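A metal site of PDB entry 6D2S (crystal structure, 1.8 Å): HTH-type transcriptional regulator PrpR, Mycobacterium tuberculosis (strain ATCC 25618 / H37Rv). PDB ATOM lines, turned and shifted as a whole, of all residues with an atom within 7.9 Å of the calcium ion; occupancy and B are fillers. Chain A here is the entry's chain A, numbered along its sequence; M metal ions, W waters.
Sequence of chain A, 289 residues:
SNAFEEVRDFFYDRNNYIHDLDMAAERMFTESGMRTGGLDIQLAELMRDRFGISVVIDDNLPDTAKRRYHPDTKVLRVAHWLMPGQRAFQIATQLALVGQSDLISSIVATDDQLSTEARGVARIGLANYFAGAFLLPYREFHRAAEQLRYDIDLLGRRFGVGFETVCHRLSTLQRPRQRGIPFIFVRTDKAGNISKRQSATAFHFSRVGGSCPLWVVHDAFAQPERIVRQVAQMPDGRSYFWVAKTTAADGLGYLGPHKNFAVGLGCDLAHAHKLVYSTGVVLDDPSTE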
ATOM      1  N   LYS A  66      25.380  21.491  -0.853  1.00  0.00           N
ATOM      2  CA  LYS A  66      25.849  21.397  -2.232  1.00  0.00           C
ATOM      3  C   LYS A  66      27.365  21.286  -2.328  1.00  0.00           C
ATOM      4  O   LYS A  66      27.885  20.895  -3.383  1.00  0.00           O
ATOM      5  CB  LYS A  66      25.378  22.605  -3.059  1.00  0.00           C
ATOM      6  CG  LYS A  66      23.864  22.677  -3.244  1.00  0.00           C
ATOM      7  CD  LYS A  66      23.473  23.815  -4.179  1.00  0.00           C
ATOM      8  CE  LYS A  66      21.963  23.856  -4.415  1.00  0.00           C
ATOM      9  NZ  LYS A  66      21.598  24.797  -5.523  1.00  0.00           N
ATOM     10  N   GLN A  86      25.531  23.863 -11.963  1.00  0.00           N
ATOM     11  CA  GLN A  86      25.593  24.082 -10.518  1.00  0.00           C
ATOM     12  C   GLN A  86      26.876  23.547  -9.909  1.00  0.00           C
ATOM     13  O   GLN A  86      27.388  24.115  -8.935  1.00  0.00           O
ATOM     14  CB  GLN A  86      24.379  23.461  -9.818  1.00  0.00           C
ATOM     15  CG  GLN A  86      23.318  24.493  -9.438  1.00  0.00           C
ATOM     16  CD  GLN A  86      23.891  25.661  -8.629  1.00  0.00           C
ATOM     17  OE1 GLN A  86      24.242  25.519  -7.451  1.00  0.00           O
ATOM     18  NE2 GLN A  86      23.990  26.827  -9.269  1.00  0.00           N
ATOM     19  N   GLY A 162      20.823  27.413 -14.707  1.00  0.00           N
ATOM     20  CA  GLY A 162      19.397  27.421 -14.439  1.00  0.00           C
ATOM     21  C   GLY A 162      18.754  28.797 -14.607  1.00  0.00           C
ATOM     22  O   GLY A 162      19.416  29.827 -14.714  1.00  0.00           O
ATOM     23  N   PHE A 163      17.417  28.772 -14.625  1.00  0.00           N
ATOM     24  CA  PHE A 163      16.606  29.957 -14.889  1.00  0.00           C
ATOM     25  C   PHE A 163      16.922  31.098 -13.912  1.00  0.00           C
ATOM     26  O   PHE A 163      17.131  32.236 -14.327  1.00  0.00           O
ATOM     27  CB  PHE A 163      15.135  29.568 -14.826  1.00  0.00           C
ATOM     28  CG  PHE A 163      14.201  30.610 -15.362  1.00  0.00           C
ATOM     29  CD1 PHE A 163      13.682  31.583 -14.530  1.00  0.00           C
ATOM     30  CD2 PHE A 163      13.826  30.609 -16.704  1.00  0.00           C
ATOM     31  CE1 PHE A 163      12.804  32.543 -15.017  1.00  0.00           C
ATOM     32  CE2 PHE A 163      12.949  31.556 -17.195  1.00  0.00           C
ATOM     33  CZ  PHE A 163      12.442  32.532 -16.345  1.00  0.00           C
ATOM     34  N   GLU A 164      16.955  30.807 -12.597  1.00  0.00           N
ATOM     35  CA  GLU A 164      17.197  31.902 -11.660  1.00  0.00           C
ATOM     36  C   GLU A 164      18.634  32.395 -11.741  1.00  0.00           C
ATOM     37  O   GLU A 164      18.904  33.568 -11.433  1.00  0.00           O
ATOM     38  CB  GLU A 164      16.848  31.501 -10.229  1.00  0.00           C
ATOM     39  CG  GLU A 164      17.765  30.464  -9.600  1.00  0.00           C
ATOM     40  CD  GLU A 164      17.296  29.032  -9.825  1.00  0.00           C
ATOM     41  OE1 GLU A 164      16.706  28.754 -10.899  1.00  0.00           O
ATOM     42  OE2 GLU A 164      17.511  28.203  -8.910  1.00  0.00           O
ATOM     43  N   THR A 165      19.581  31.533 -12.152  1.00  0.00           N
ATOM     44  CA  THR A 165      20.960  31.979 -12.321  1.00  0.00           C
ATOM     45  C   THR A 165      21.063  32.991 -13.453  1.00  0.00           C
ATOM     46  O   THR A 165      21.757  34.006 -13.314  1.00  0.00           O
ATOM     47  CB  THR A 165      21.860  30.762 -12.582  1.00  0.00           C
ATOM     48  OG1 THR A 165      21.707  29.826 -11.503  1.00  0.00           O
ATOM     49  CG2 THR A 165      23.344  31.179 -12.664  1.00  0.00           C
ATOM     50  N   GLU A 225       6.422  25.906 -14.393  1.00  0.00           N
ATOM     51  CA  GLU A 225       7.416  25.711 -15.444  1.00  0.00           C
ATOM     52  C   GLU A 225       7.006  26.332 -16.772  1.00  0.00           C
ATOM     53  O   GLU A 225       7.592  26.016 -17.821  1.00  0.00           O
ATOM     54  CB  GLU A 225       7.749  24.224 -15.607  1.00  0.00           C
ATOM     55  CG  GLU A 225       8.314  23.630 -14.324  1.00  0.00           C
ATOM     56  CD  GLU A 225       9.079  22.344 -14.544  1.00  0.00           C
ATOM     57  OE1 GLU A 225       8.963  21.758 -15.644  1.00  0.00           O
ATOM     58  OE2 GLU A 225       9.813  21.931 -13.623  1.00  0.00           O
ATOM     59  N   THR A 246       8.337  29.532 -12.371  1.00  0.00           N
ATOM     60  CA  THR A 246       8.777  28.722 -11.248  1.00  0.00           C
ATOM     61  C   THR A 246      10.111  28.077 -11.588  1.00  0.00           C
ATOM     62  O   THR A 246      10.452  27.878 -12.754  1.00  0.00           O
ATOM     63  CB  THR A 246       7.756  27.635 -10.882  1.00  0.00           C
ATOM     64  OG1 THR A 246       7.531  26.788 -12.016  1.00  0.00           O
ATOM     65  CG2 THR A 246       6.436  28.247 -10.435  1.00  0.00           C
ATOM     66  N   THR A 247      10.870  27.767 -10.544  1.00  0.00           N
ATOM     67  CA  THR A 247      12.133  27.059 -10.681  1.00  0.00           C
ATOM     68  C   THR A 247      11.899  25.604 -10.320  1.00  0.00           C
ATOM     69  O   THR A 247      11.278  25.302  -9.293  1.00  0.00           O
ATOM     70  CB  THR A 247      13.203  27.662  -9.770  1.00  0.00           C
ATOM     71  OG1 THR A 247      12.896  27.340  -8.411  1.00  0.00           O
ATOM     72  CG2 THR A 247      13.221  29.172  -9.937  1.00  0.00           C
ATOM     73  N   ALA A 248      12.382  24.698 -11.167  1.00  0.00           N
ATOM     74  CA  ALA A 248      12.278  23.277 -10.853  1.00  0.00           C
ATOM     75  C   ALA A 248      13.204  22.940  -9.688  1.00  0.00           C
ATOM     76  O   ALA A 248      14.355  23.387  -9.651  1.00  0.00           O
ATOM     77  CB  ALA A 248      12.627  22.438 -12.082  1.00  0.00           C
ATOM     78  N   ALA A 249      12.694  22.159  -8.733  1.00  0.00           N
ATOM     79  CA  ALA A 249      13.480  21.688  -7.595  1.00  0.00           C
ATOM     80  C   ALA A 249      14.306  20.496  -8.062  1.00  0.00           C
ATOM     81  O   ALA A 249      13.857  19.355  -8.042  1.00  0.00           O
ATOM     82  CB  ALA A 249      12.577  21.326  -6.422  1.00  0.00           C
ATOM     83  N   ASP A 250      15.538  20.780  -8.489  1.00  0.00           N
ATOM     84  CA  ASP A 250      16.377  19.776  -9.122  1.00  0.00           C
ATOM     85  C   ASP A 250      17.851  20.135  -8.945  1.00  0.00           C
ATOM     86  O   ASP A 250      18.223  20.754  -7.945  1.00  0.00           O
ATOM     87  CB  ASP A 250      16.016  19.642 -10.598  1.00  0.00           C
ATOM     88  CG  ASP A 250      16.258  20.918 -11.381  1.00  0.00           C
ATOM     89  OD1 ASP A 250      16.091  20.896 -12.615  1.00  0.00           O
ATOM     90  OD2 ASP A 250      16.628  21.935 -10.743  1.00  0.00           O
ATOM     91  N   GLY A 251      18.689  19.762  -9.908  1.00  0.00           N
ATOM     92  CA  GLY A 251      20.117  19.986  -9.822  1.00  0.00           C
ATOM     93  C   GLY A 251      20.646  21.240 -10.502  1.00  0.00           C
ATOM     94  O   GLY A 251      21.863  21.409 -10.594  1.00  0.00           O
ATOM     95  N   LEU A 252      19.779  22.127 -10.987  1.00  0.00           N
ATOM     96  CA  LEU A 252      20.225  23.319 -11.675  1.00  0.00           C
ATOM     97  C   LEU A 252      19.654  24.559 -10.991  1.00  0.00           C
ATOM     98  O   LEU A 252      18.610  24.494 -10.340  1.00  0.00           O
ATOM     99  CB  LEU A 252      19.793  23.281 -13.147  1.00  0.00           C
ATOM    100  CG  LEU A 252      20.645  24.027 -14.172  1.00  0.00           C
ATOM    101  CD1 LEU A 252      22.109  23.617 -14.081  1.00  0.00           C
ATOM    102  CD2 LEU A 252      20.102  23.760 -15.573  1.00  0.00           C
ATOM    103  N   GLY A 253      20.346  25.677 -11.152  1.00  0.00           N
ATOM    104  CA  GLY A 253      19.959  26.910 -10.479  1.00  0.00           C
ATOM    105  C   GLY A 253      20.485  26.972  -9.054  1.00  0.00           C
ATOM    106  O   GLY A 253      20.640  25.935  -8.405  1.00  0.00           O
ATOM    107  N   TYR A 254      20.743  28.176  -8.552  1.00  0.00           N
ATOM    108  CA  TYR A 254      21.336  28.295  -7.223  1.00  0.00           C
ATOM    109  C   TYR A 254      20.326  28.159  -6.102  1.00  0.00           C
ATOM    110  O   TYR A 254      20.734  27.969  -4.955  1.00  0.00           O
ATOM    111  CB  TYR A 254      22.086  29.639  -7.071  1.00  0.00           C
ATOM    112  CG  TYR A 254      21.202  30.878  -7.189  1.00  0.00           C
ATOM    113  CD1 TYR A 254      20.463  31.332  -6.089  1.00  0.00           C
ATOM    114  CD2 TYR A 254      21.128  31.593  -8.372  1.00  0.00           C
ATOM    115  CE1 TYR A 254      19.657  32.457  -6.196  1.00  0.00           C
ATOM    116  CE2 TYR A 254      20.329  32.725  -8.479  1.00  0.00           C
ATOM    117  CZ  TYR A 254      19.596  33.148  -7.399  1.00  0.00           C
ATOM    118  OH  TYR A 254      18.806  34.273  -7.500  1.00  0.00           O
ATOM    119  N   LEU A 255      19.030  28.231  -6.382  1.00  0.00           N
ATOM    120  CA  LEU A 255      18.037  28.116  -5.316  1.00  0.00           C
ATOM    121  C   LEU A 255      17.929  26.666  -4.856  1.00  0.00           C
ATOM    122  O   LEU A 255      17.857  25.748  -5.669  1.00  0.00           O
ATOM    123  CB  LEU A 255      16.682  28.653  -5.771  1.00  0.00           C
ATOM    124  CG  LEU A 255      16.648  30.181  -5.906  1.00  0.00           C
ATOM    125  CD1 LEU A 255      15.392  30.664  -6.623  1.00  0.00           C
ATOM    126  CD2 LEU A 255      16.767  30.854  -4.538  1.00  0.00           C
ATOM    127  N   GLY A 256      17.938  26.460  -3.534  1.00  0.00           N
ATOM    128  CA  GLY A 256      17.910  25.143  -2.974  1.00  0.00           C
ATOM    129  C   GLY A 256      16.705  24.347  -3.440  1.00  0.00           C
ATOM    130  O   GLY A 256      15.615  24.886  -3.639  1.00  0.00           O
ATOM    131  N   PRO A 257      16.889  23.043  -3.640  1.00  0.00           N
ATOM    132  CA  PRO A 257      15.771  22.181  -4.022  1.00  0.00           C
ATOM    133  C   PRO A 257      14.828  21.837  -2.874  1.00  0.00           C
ATOM    134  O   PRO A 257      13.932  21.008  -3.074  1.00  0.00           O
ATOM    135  CB  PRO A 257      16.488  20.920  -4.532  1.00  0.00           C
ATOM    136  CG  PRO A 257      17.718  20.849  -3.690  1.00  0.00           C
ATOM    137  CD  PRO A 257      18.149  22.287  -3.495  1.00  0.00           C
ATOM    138  N   LYS A 259      12.486  23.573  -1.563  1.00  0.00           N
ATOM    139  CA  LYS A 259      11.117  24.028  -1.784  1.00  0.00           C
ATOM    140  C   LYS A 259      11.053  24.741  -3.133  1.00  0.00           C
ATOM    141  O   LYS A 259      12.066  24.960  -3.793  1.00  0.00           O
ATOM    142  CB  LYS A 259      10.628  24.926  -0.645  1.00  0.00           C
ATOM    143  CG  LYS A 259      11.531  26.102  -0.313  1.00  0.00           C
ATOM    144  CD  LYS A 259      11.021  26.802   0.938  1.00  0.00           C
ATOM    145  CE  LYS A 259      11.743  28.109   1.200  1.00  0.00           C
ATOM    146  NZ  LYS A 259      11.253  28.754   2.443  1.00  0.00           N
HETATM  147 CA    CA M   1      16.347  24.330 -10.346  1.00  0.00          CA
HETATM  148  O   HOH W   1      16.076  26.071  -8.849  1.00  0.00           O
HETATM  149  O   HOH W   2      17.188  22.794  -8.412  1.00  0.00           O
HETATM  150  O   HOH W   3      16.335  23.326 -13.166  1.00  0.00           O
HETATM  151  O   HOH W   4      16.472  26.289 -11.786  1.00  0.00           O
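Of the 20 residues printed, 3 come within 4 Å of the calcium ion.
The nearest printed residue that does not touch the calcium ion is Glu 164 (4.3 Å).
Water W1 bridges OE2 of Glu 164 and OG1 of Thr 247.
The calcium ion is bound by O of Leu 252 (2.3 Å), O of Ala 248 (2.3 Å), water W1 (2.3 Å), water W4 (2.4 Å), OD2 of Asp 250 (2.4 Å) and water W2 (2.6 Å).
The calcium ion has six donor atoms within binding distance.
Slightly farther from the calcium ion lies water W3 (3.0 Å).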
